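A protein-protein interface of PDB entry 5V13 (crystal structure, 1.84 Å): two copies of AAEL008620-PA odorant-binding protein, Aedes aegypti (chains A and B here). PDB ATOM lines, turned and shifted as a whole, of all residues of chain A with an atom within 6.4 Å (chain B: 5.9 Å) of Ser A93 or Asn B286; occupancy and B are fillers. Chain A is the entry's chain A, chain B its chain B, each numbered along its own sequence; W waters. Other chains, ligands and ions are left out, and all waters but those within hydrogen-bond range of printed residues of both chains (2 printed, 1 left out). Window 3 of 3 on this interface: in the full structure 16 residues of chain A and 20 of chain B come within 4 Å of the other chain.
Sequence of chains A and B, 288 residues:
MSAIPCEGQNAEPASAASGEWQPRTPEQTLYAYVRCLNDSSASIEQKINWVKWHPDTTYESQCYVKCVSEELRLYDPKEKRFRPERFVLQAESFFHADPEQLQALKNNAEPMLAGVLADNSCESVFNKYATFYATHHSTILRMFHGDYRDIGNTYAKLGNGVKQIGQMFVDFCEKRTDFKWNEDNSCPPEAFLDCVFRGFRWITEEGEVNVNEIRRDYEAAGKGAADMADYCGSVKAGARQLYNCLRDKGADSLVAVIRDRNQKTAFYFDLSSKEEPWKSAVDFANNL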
ATOM      1  N   PRO A  23      12.589   5.357 -31.131  1.00  0.00           N
ATOM      2  CA  PRO A  23      12.259   6.728 -30.716  1.00  0.00           C
ATOM      3  C   PRO A  23      11.374   7.416 -31.746  1.00  0.00           C
ATOM      4  O   PRO A  23      11.580   7.284 -32.958  1.00  0.00           O
ATOM      5  CB  PRO A  23      13.635   7.409 -30.612  1.00  0.00           C
ATOM      6  CG  PRO A  23      14.572   6.285 -30.321  1.00  0.00           C
ATOM      7  CD  PRO A  23      14.040   5.103 -31.088  1.00  0.00           C
ATOM      8  N   VAL A  88      12.623   6.412 -21.632  1.00  0.00           N
ATOM      9  CA  VAL A  88      14.078   6.440 -21.478  1.00  0.00           C
ATOM     10  C   VAL A  88      14.754   6.447 -22.840  1.00  0.00           C
ATOM     11  O   VAL A  88      15.702   7.208 -23.087  1.00  0.00           O
ATOM     12  CB  VAL A  88      14.558   5.253 -20.623  1.00  0.00           C
ATOM     13  CG1 VAL A  88      16.093   5.093 -20.732  1.00  0.00           C
ATOM     14  CG2 VAL A  88      14.165   5.456 -19.178  1.00  0.00           C
ATOM     15  N   LEU A  89      14.284   5.586 -23.747  1.00  0.00           N
ATOM     16  CA  LEU A  89      14.897   5.518 -25.066  1.00  0.00           C
ATOM     17  C   LEU A  89      14.690   6.821 -25.826  1.00  0.00           C
ATOM     18  O   LEU A  89      15.589   7.281 -26.543  1.00  0.00           O
ATOM     19  CB  LEU A  89      14.346   4.313 -25.839  1.00  0.00           C
ATOM     20  CG  LEU A  89      15.163   3.839 -27.045  1.00  0.00           C
ATOM     21  CD1 LEU A  89      16.502   3.176 -26.628  1.00  0.00           C
ATOM     22  CD2 LEU A  89      14.330   2.919 -27.942  1.00  0.00           C
ATOM     23  N   GLN A  90      13.522   7.454 -25.654  1.00  0.00           N
ATOM     24  CA  GLN A  90      13.283   8.752 -26.277  1.00  0.00           C
ATOM     25  C   GLN A  90      14.236   9.811 -25.737  1.00  0.00           C
ATOM     26  O   GLN A  90      14.770  10.623 -26.503  1.00  0.00           O
ATOM     27  CB  GLN A  90      11.837   9.201 -26.051  1.00  0.00           C
ATOM     28  CG  GLN A  90      11.415  10.428 -26.873  1.00  0.00           C
ATOM     29  CD  GLN A  90      11.073  10.064 -28.317  1.00  0.00           C
ATOM     30  OE1 GLN A  90      10.739   8.921 -28.615  1.00  0.00           O
ATOM     31  NE2 GLN A  90      11.169  11.041 -29.224  1.00  0.00           N
ATOM     32  N   ALA A  91      14.444   9.831 -24.420  1.00  0.00           N
ATOM     33  CA  ALA A  91      15.337  10.825 -23.836  1.00  0.00           C
ATOM     34  C   ALA A  91      16.776  10.608 -24.285  1.00  0.00           C
ATOM     35  O   ALA A  91      17.497  11.571 -24.569  1.00  0.00           O
ATOM     36  CB  ALA A  91      15.245  10.789 -22.314  1.00  0.00           C
ATOM     37  N   GLU A  92      17.209   9.352 -24.366  1.00  0.00           N
ATOM     38  CA  GLU A  92      18.577   9.080 -24.805  1.00  0.00           C
ATOM     39  C   GLU A  92      18.824   9.554 -26.233  1.00  0.00           C
ATOM     40  O   GLU A  92      19.935   9.985 -26.564  1.00  0.00           O
ATOM     41  CB  GLU A  92      18.871   7.588 -24.670  1.00  0.00           C
ATOM     42  CG  GLU A  92      18.955   7.126 -23.221  1.00  0.00           C
ATOM     43  CD  GLU A  92      19.129   5.614 -23.066  1.00  0.00           C
ATOM     44  OE1 GLU A  92      19.497   5.166 -21.954  1.00  0.00           O
ATOM     45  OE2 GLU A  92      18.877   4.873 -24.039  1.00  0.00           O
ATOM     46  N   SER A  93      17.804   9.496 -27.088  1.00  0.00           N
ATOM     47  CA  SER A  93      17.977   9.896 -28.477  1.00  0.00           C
ATOM     48  C   SER A  93      17.880  11.404 -28.668  1.00  0.00           C
ATOM     49  O   SER A  93      18.575  11.957 -29.530  1.00  0.00           O
ATOM     50  CB  SER A  93      16.943   9.192 -29.363  1.00  0.00           C
ATOM     51  OG  SER A  93      17.022   9.670 -30.698  1.00  0.00           O
ATOM     52  N   PHE A  94      17.026  12.090 -27.900  1.00  0.00           N
ATOM     53  CA  PHE A  94      16.637  13.456 -28.250  1.00  0.00           C
ATOM     54  C   PHE A  94      16.757  14.499 -27.145  1.00  0.00           C
ATOM     55  O   PHE A  94      16.369  15.649 -27.376  1.00  0.00           O
ATOM     56  CB  PHE A  94      15.192  13.493 -28.773  1.00  0.00           C
ATOM     57  CG  PHE A  94      15.010  12.856 -30.139  1.00  0.00           C
ATOM     58  CD1 PHE A  94      15.650  13.375 -31.258  1.00  0.00           C
ATOM     59  CD2 PHE A  94      14.188  11.752 -30.300  1.00  0.00           C
ATOM     60  CE1 PHE A  94      15.494  12.782 -32.510  1.00  0.00           C
ATOM     61  CE2 PHE A  94      14.007  11.165 -31.545  1.00  0.00           C
ATOM     62  CZ  PHE A  94      14.664  11.685 -32.659  1.00  0.00           C
ATOM     63  N   PHE A  95      17.260  14.159 -25.962  1.00  0.00           N
ATOM     64  CA  PHE A  95      17.449  15.162 -24.912  1.00  0.00           C
ATOM     65  C   PHE A  95      18.939  15.304 -24.619  1.00  0.00           C
ATOM     66  O   PHE A  95      19.537  14.430 -23.981  1.00  0.00           O
ATOM     67  CB  PHE A  95      16.679  14.811 -23.639  1.00  0.00           C
ATOM     68  CG  PHE A  95      16.787  15.870 -22.579  1.00  0.00           C
ATOM     69  CD1 PHE A  95      16.066  17.049 -22.690  1.00  0.00           C
ATOM     70  CD2 PHE A  95      17.623  15.700 -21.495  1.00  0.00           C
ATOM     71  CE1 PHE A  95      16.172  18.039 -21.725  1.00  0.00           C
ATOM     72  CE2 PHE A  95      17.735  16.680 -20.524  1.00  0.00           C
ATOM     73  CZ  PHE A  95      17.008  17.854 -20.639  1.00  0.00           C
ATOM     74  N   HIS A  96      19.531  16.421 -25.064  1.00  0.00           N
ATOM     75  CA  HIS A  96      20.956  16.684 -24.878  1.00  0.00           C
ATOM     76  C   HIS A  96      21.231  17.971 -24.113  1.00  0.00           C
ATOM     77  O   HIS A  96      22.393  18.394 -24.032  1.00  0.00           O
ATOM     78  CB  HIS A  96      21.652  16.737 -26.238  1.00  0.00           C
ATOM     79  CG  HIS A  96      21.103  15.749 -27.217  1.00  0.00           C
ATOM     80  ND1 HIS A  96      21.171  14.387 -27.010  1.00  0.00           N
ATOM     81  CD2 HIS A  96      20.445  15.922 -28.389  1.00  0.00           C
ATOM     82  CE1 HIS A  96      20.590  13.762 -28.021  1.00  0.00           C
ATOM     83  NE2 HIS A  96      20.141  14.671 -28.870  1.00  0.00           N
ATOM     84  N   LYS A 157      19.714  15.126 -38.585  1.00  0.00           N
ATOM     85  CA  LYS A 157      20.232  13.847 -38.093  1.00  0.00           C
ATOM     86  C   LYS A 157      19.448  12.684 -38.675  1.00  0.00           C
ATOM     87  O   LYS A 157      20.011  11.626 -38.963  1.00  0.00           O
ATOM     88  CB  LYS A 157      20.184  13.822 -36.563  1.00  0.00           C
ATOM     89  CG  LYS A 157      20.757  12.563 -35.928  1.00  0.00           C
ATOM     90  CD  LYS A 157      20.518  12.525 -34.409  1.00  0.00           C
ATOM     91  CE  LYS A 157      19.057  12.206 -34.060  1.00  0.00           C
ATOM     92  NZ  LYS A 157      18.833  11.977 -32.590  1.00  0.00           N
ATOM     93  N   GLY B 146      32.099  16.514 -36.070  1.00  0.00           N
ATOM     94  CA  GLY B 146      32.028  15.590 -34.953  1.00  0.00           C
ATOM     95  C   GLY B 146      31.033  15.963 -33.869  1.00  0.00           C
ATOM     96  O   GLY B 146      30.744  15.141 -32.996  1.00  0.00           O
ATOM     97  N   TYR B 148      27.250  17.071 -33.032  1.00  0.00           N
ATOM     98  CA  TYR B 148      25.934  17.137 -33.669  1.00  0.00           C
ATOM     99  C   TYR B 148      25.143  18.386 -33.296  1.00  0.00           C
ATOM    100  O   TYR B 148      24.045  18.579 -33.823  1.00  0.00           O
ATOM    101  CB  TYR B 148      25.125  15.880 -33.343  1.00  0.00           C
ATOM    102  CG  TYR B 148      25.653  14.655 -34.069  1.00  0.00           C
ATOM    103  CD1 TYR B 148      26.624  14.781 -35.059  1.00  0.00           C
ATOM    104  CD2 TYR B 148      25.181  13.383 -33.770  1.00  0.00           C
ATOM    105  CE1 TYR B 148      27.115  13.675 -35.729  1.00  0.00           C
ATOM    106  CE2 TYR B 148      25.664  12.271 -34.432  1.00  0.00           C
ATOM    107  CZ  TYR B 148      26.629  12.421 -35.413  1.00  0.00           C
ATOM    108  OH  TYR B 148      27.114  11.316 -36.079  1.00  0.00           O
ATOM    109  N   ARG B 149      25.658  19.247 -32.416  1.00  0.00           N
ATOM    110  CA  ARG B 149      24.992  20.524 -32.182  1.00  0.00           C
ATOM    111  C   ARG B 149      24.922  21.377 -33.445  1.00  0.00           C
ATOM    112  O   ARG B 149      24.047  22.251 -33.549  1.00  0.00           O
ATOM    113  CB  ARG B 149      25.714  21.289 -31.071  1.00  0.00           C
ATOM    114  CG  ARG B 149      25.316  20.817 -29.672  1.00  0.00           C
ATOM    115  CD  ARG B 149      26.066  21.557 -28.584  1.00  0.00           C
ATOM    116  NE  ARG B 149      27.508  21.453 -28.766  1.00  0.00           N
ATOM    117  CZ  ARG B 149      28.409  21.994 -27.953  1.00  0.00           C
ATOM    118  NH1 ARG B 149      28.013  22.676 -26.882  1.00  0.00           N
ATOM    119  NH2 ARG B 149      29.704  21.850 -28.208  1.00  0.00           N
ATOM    120  N   ALA B 281      29.505   6.091 -30.767  1.00  0.00           N
ATOM    121  CA  ALA B 281      29.752   7.205 -31.686  1.00  0.00           C
ATOM    122  C   ALA B 281      28.610   8.211 -31.627  1.00  0.00           C
ATOM    123  O   ALA B 281      28.837   9.426 -31.535  1.00  0.00           O
ATOM    124  CB  ALA B 281      29.932   6.693 -33.108  1.00  0.00           C
ATOM    125  N   VAL B 282      27.374   7.710 -31.629  1.00  0.00           N
ATOM    126  CA  VAL B 282      26.203   8.583 -31.622  1.00  0.00           C
ATOM    127  C   VAL B 282      26.049   9.282 -30.274  1.00  0.00           C
ATOM    128  O   VAL B 282      25.749  10.481 -30.213  1.00  0.00           O
ATOM    129  CB  VAL B 282      24.945   7.773 -31.978  1.00  0.00           C
ATOM    130  CG1 VAL B 282      23.697   8.648 -31.845  1.00  0.00           C
ATOM    131  CG2 VAL B 282      25.073   7.184 -33.368  1.00  0.00           C
ATOM    132  N   ASP B 283      26.235   8.549 -29.171  1.00  0.00           N
ATOM    133  CA  ASP B 283      26.038   9.151 -27.855  1.00  0.00           C
ATOM    134  C   ASP B 283      27.050  10.252 -27.592  1.00  0.00           C
ATOM    135  O   ASP B 283      26.730  11.261 -26.949  1.00  0.00           O
ATOM    136  CB  ASP B 283      26.132   8.089 -26.759  1.00  0.00           C
ATOM    137  CG  ASP B 283      25.009   7.083 -26.830  1.00  0.00           C
ATOM    138  OD1 ASP B 283      23.926   7.439 -27.349  1.00  0.00           O
ATOM    139  OD2 ASP B 283      25.213   5.937 -26.367  1.00  0.00           O
ATOM    140  N   PHE B 284      28.287  10.064 -28.057  1.00  0.00           N
ATOM    141  CA  PHE B 284      29.315  11.076 -27.841  1.00  0.00           C
ATOM    142  C   PHE B 284      29.016  12.333 -28.646  1.00  0.00           C
ATOM    143  O   PHE B 284      29.110  13.454 -28.132  1.00  0.00           O
ATOM    144  CB  PHE B 284      30.697  10.522 -28.216  1.00  0.00           C
ATOM    145  CG  PHE B 284      31.806  11.532 -28.089  1.00  0.00           C
ATOM    146  CD1 PHE B 284      32.485  11.683 -26.893  1.00  0.00           C
ATOM    147  CD2 PHE B 284      32.162  12.339 -29.166  1.00  0.00           C
ATOM    148  CE1 PHE B 284      33.500  12.611 -26.773  1.00  0.00           C
ATOM    149  CE2 PHE B 284      33.173  13.272 -29.045  1.00  0.00           C
ATOM    150  CZ  PHE B 284      33.844  13.403 -27.847  1.00  0.00           C
ATOM    151  N   ALA B 285      28.662  12.163 -29.918  1.00  0.00           N
ATOM    152  CA  ALA B 285      28.462  13.317 -30.791  1.00  0.00           C
ATOM    153  C   ALA B 285      27.184  14.070 -30.440  1.00  0.00           C
ATOM    154  O   ALA B 285      27.077  15.274 -30.711  1.00  0.00           O
ATOM    155  CB  ALA B 285      28.425  12.862 -32.245  1.00  0.00           C
ATOM    156  N   ASN B 286      26.214  13.377 -29.846  1.00  0.00           N
ATOM    157  CA  ASN B 286      24.953  13.983 -29.449  1.00  0.00           C
ATOM    158  C   ASN B 286      25.074  14.850 -28.210  1.00  0.00           C
ATOM    159  O   ASN B 286      24.202  15.697 -27.980  1.00  0.00           O
ATOM    160  CB  ASN B 286      23.905  12.904 -29.162  1.00  0.00           C
ATOM    161  CG  ASN B 286      23.052  12.578 -30.362  1.00  0.00           C
ATOM    162  OD1 ASN B 286      23.115  13.253 -31.388  1.00  0.00           O
ATOM    163  ND2 ASN B 286      22.226  11.541 -30.232  1.00  0.00           N
ATOM    164  N   ASN B 287      26.102  14.649 -27.389  1.00  0.00           N
ATOM    165  CA  ASN B 287      26.051  15.189 -26.038  1.00  0.00           C
ATOM    166  C   ASN B 287      27.314  15.957 -25.681  1.00  0.00           C
ATOM    167  O   ASN B 287      27.778  15.917 -24.539  1.00  0.00           O
ATOM    168  CB  ASN B 287      25.784  14.073 -25.026  1.00  0.00           C
ATOM    169  CG  ASN B 287      24.387  13.480 -25.170  1.00  0.00           C
ATOM    170  OD1 ASN B 287      23.401  14.069 -24.726  1.00  0.00           O
ATOM    171  ND2 ASN B 287      24.298  12.315 -25.804  1.00  0.00           N
ATOM    172  N   LEU B 288      27.874  16.703 -26.630  1.00  0.00           N
ATOM    173  CA  LEU B 288      28.973  17.608 -26.294  1.00  0.00           C
ATOM    174  C   LEU B 288      28.442  18.933 -25.758  1.00  0.00           C
ATOM    175  O   LEU B 288      29.134  19.620 -25.007  1.00  0.00           O
ATOM    176  CB  LEU B 288      29.863  17.858 -27.502  1.00  0.00           C
ATOM    177  CG  LEU B 288      30.595  16.622 -28.012  1.00  0.00           C
ATOM    178  CD1 LEU B 288      31.329  16.981 -29.264  1.00  0.00           C
ATOM    179  CD2 LEU B 288      31.551  16.081 -26.954  1.00  0.00           C
HETATM  180  O   HOH W   1      20.534   9.764 -31.668  1.00  0.00           O
HETATM  181  O   HOH W   2      22.363  10.089 -27.482  1.00  0.00           O
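The backbone carbonyl oxygen (O) of Asn B286 sits close to a ring nitrogen (ND1) of His A96 (3.4 Å). OD1 of Asn B287 is in hydrogen-bond range of ND1 of His A96, 3.2 Å away.
The backbone carbonyl oxygen (O) of Ser A93 sits close to a ring nitrogen (NE2) of His A96 (3.2 Å). O of Asp B283 sits at hydrogen-bond distance from ND2 of Asn B287. NZ of Lys A157 sits at hydrogen-bond distance from O of Ser A93, at 3.1 Å.
Among the printed residues, pairs that only touch across the chains: Ser A93 with Asn B286 and Phe A95 with Asn B287.
Ala A91 touches none of the printed residues of chain B. Ser A93 touches just one residue of chain B: Asn B286. Of the printed residues of chain B, Phe A95 touches Asn B287. Of the printed residues of chain B, His A96 touches Asn B286 and Asn B287. Of chain A, only Ser A93 and His A96 come within 4 Å of Asn B286. The nearest printed residue of chain B that does not touch Ser A93 is Asp B283 (6.5 Å). The nearest residue of chain A that does not touch Asn B286 is Lys A157 (4.05 Å). The nearest printed residue of chain B that does not touch Phe A95 is Asn B286 (6.3 Å).
Along chain B the printed residues that touch a printed residue of chain A span positions 286 to 287. Among the printed residues, 4 pairs touch across the chains. Among the printed residues, no Asp or Glu carboxylate lies within 4 Å of a Lys or Arg side-chain nitrogen of the other chain.
No position is printed for both chains.
Water W2 lies within hydrogen-bond range of O of Glu A92 (2.6 Å), OD1 of Asp B283 (3.1 Å), ND2 of Asn B286 (3.1 Å) and ND2 of Asn B287 (3.4 Å). Water W1 bridges ND2 of Asn B286 (2.8 Å) and NZ of Lys A157 (2.9 Å).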
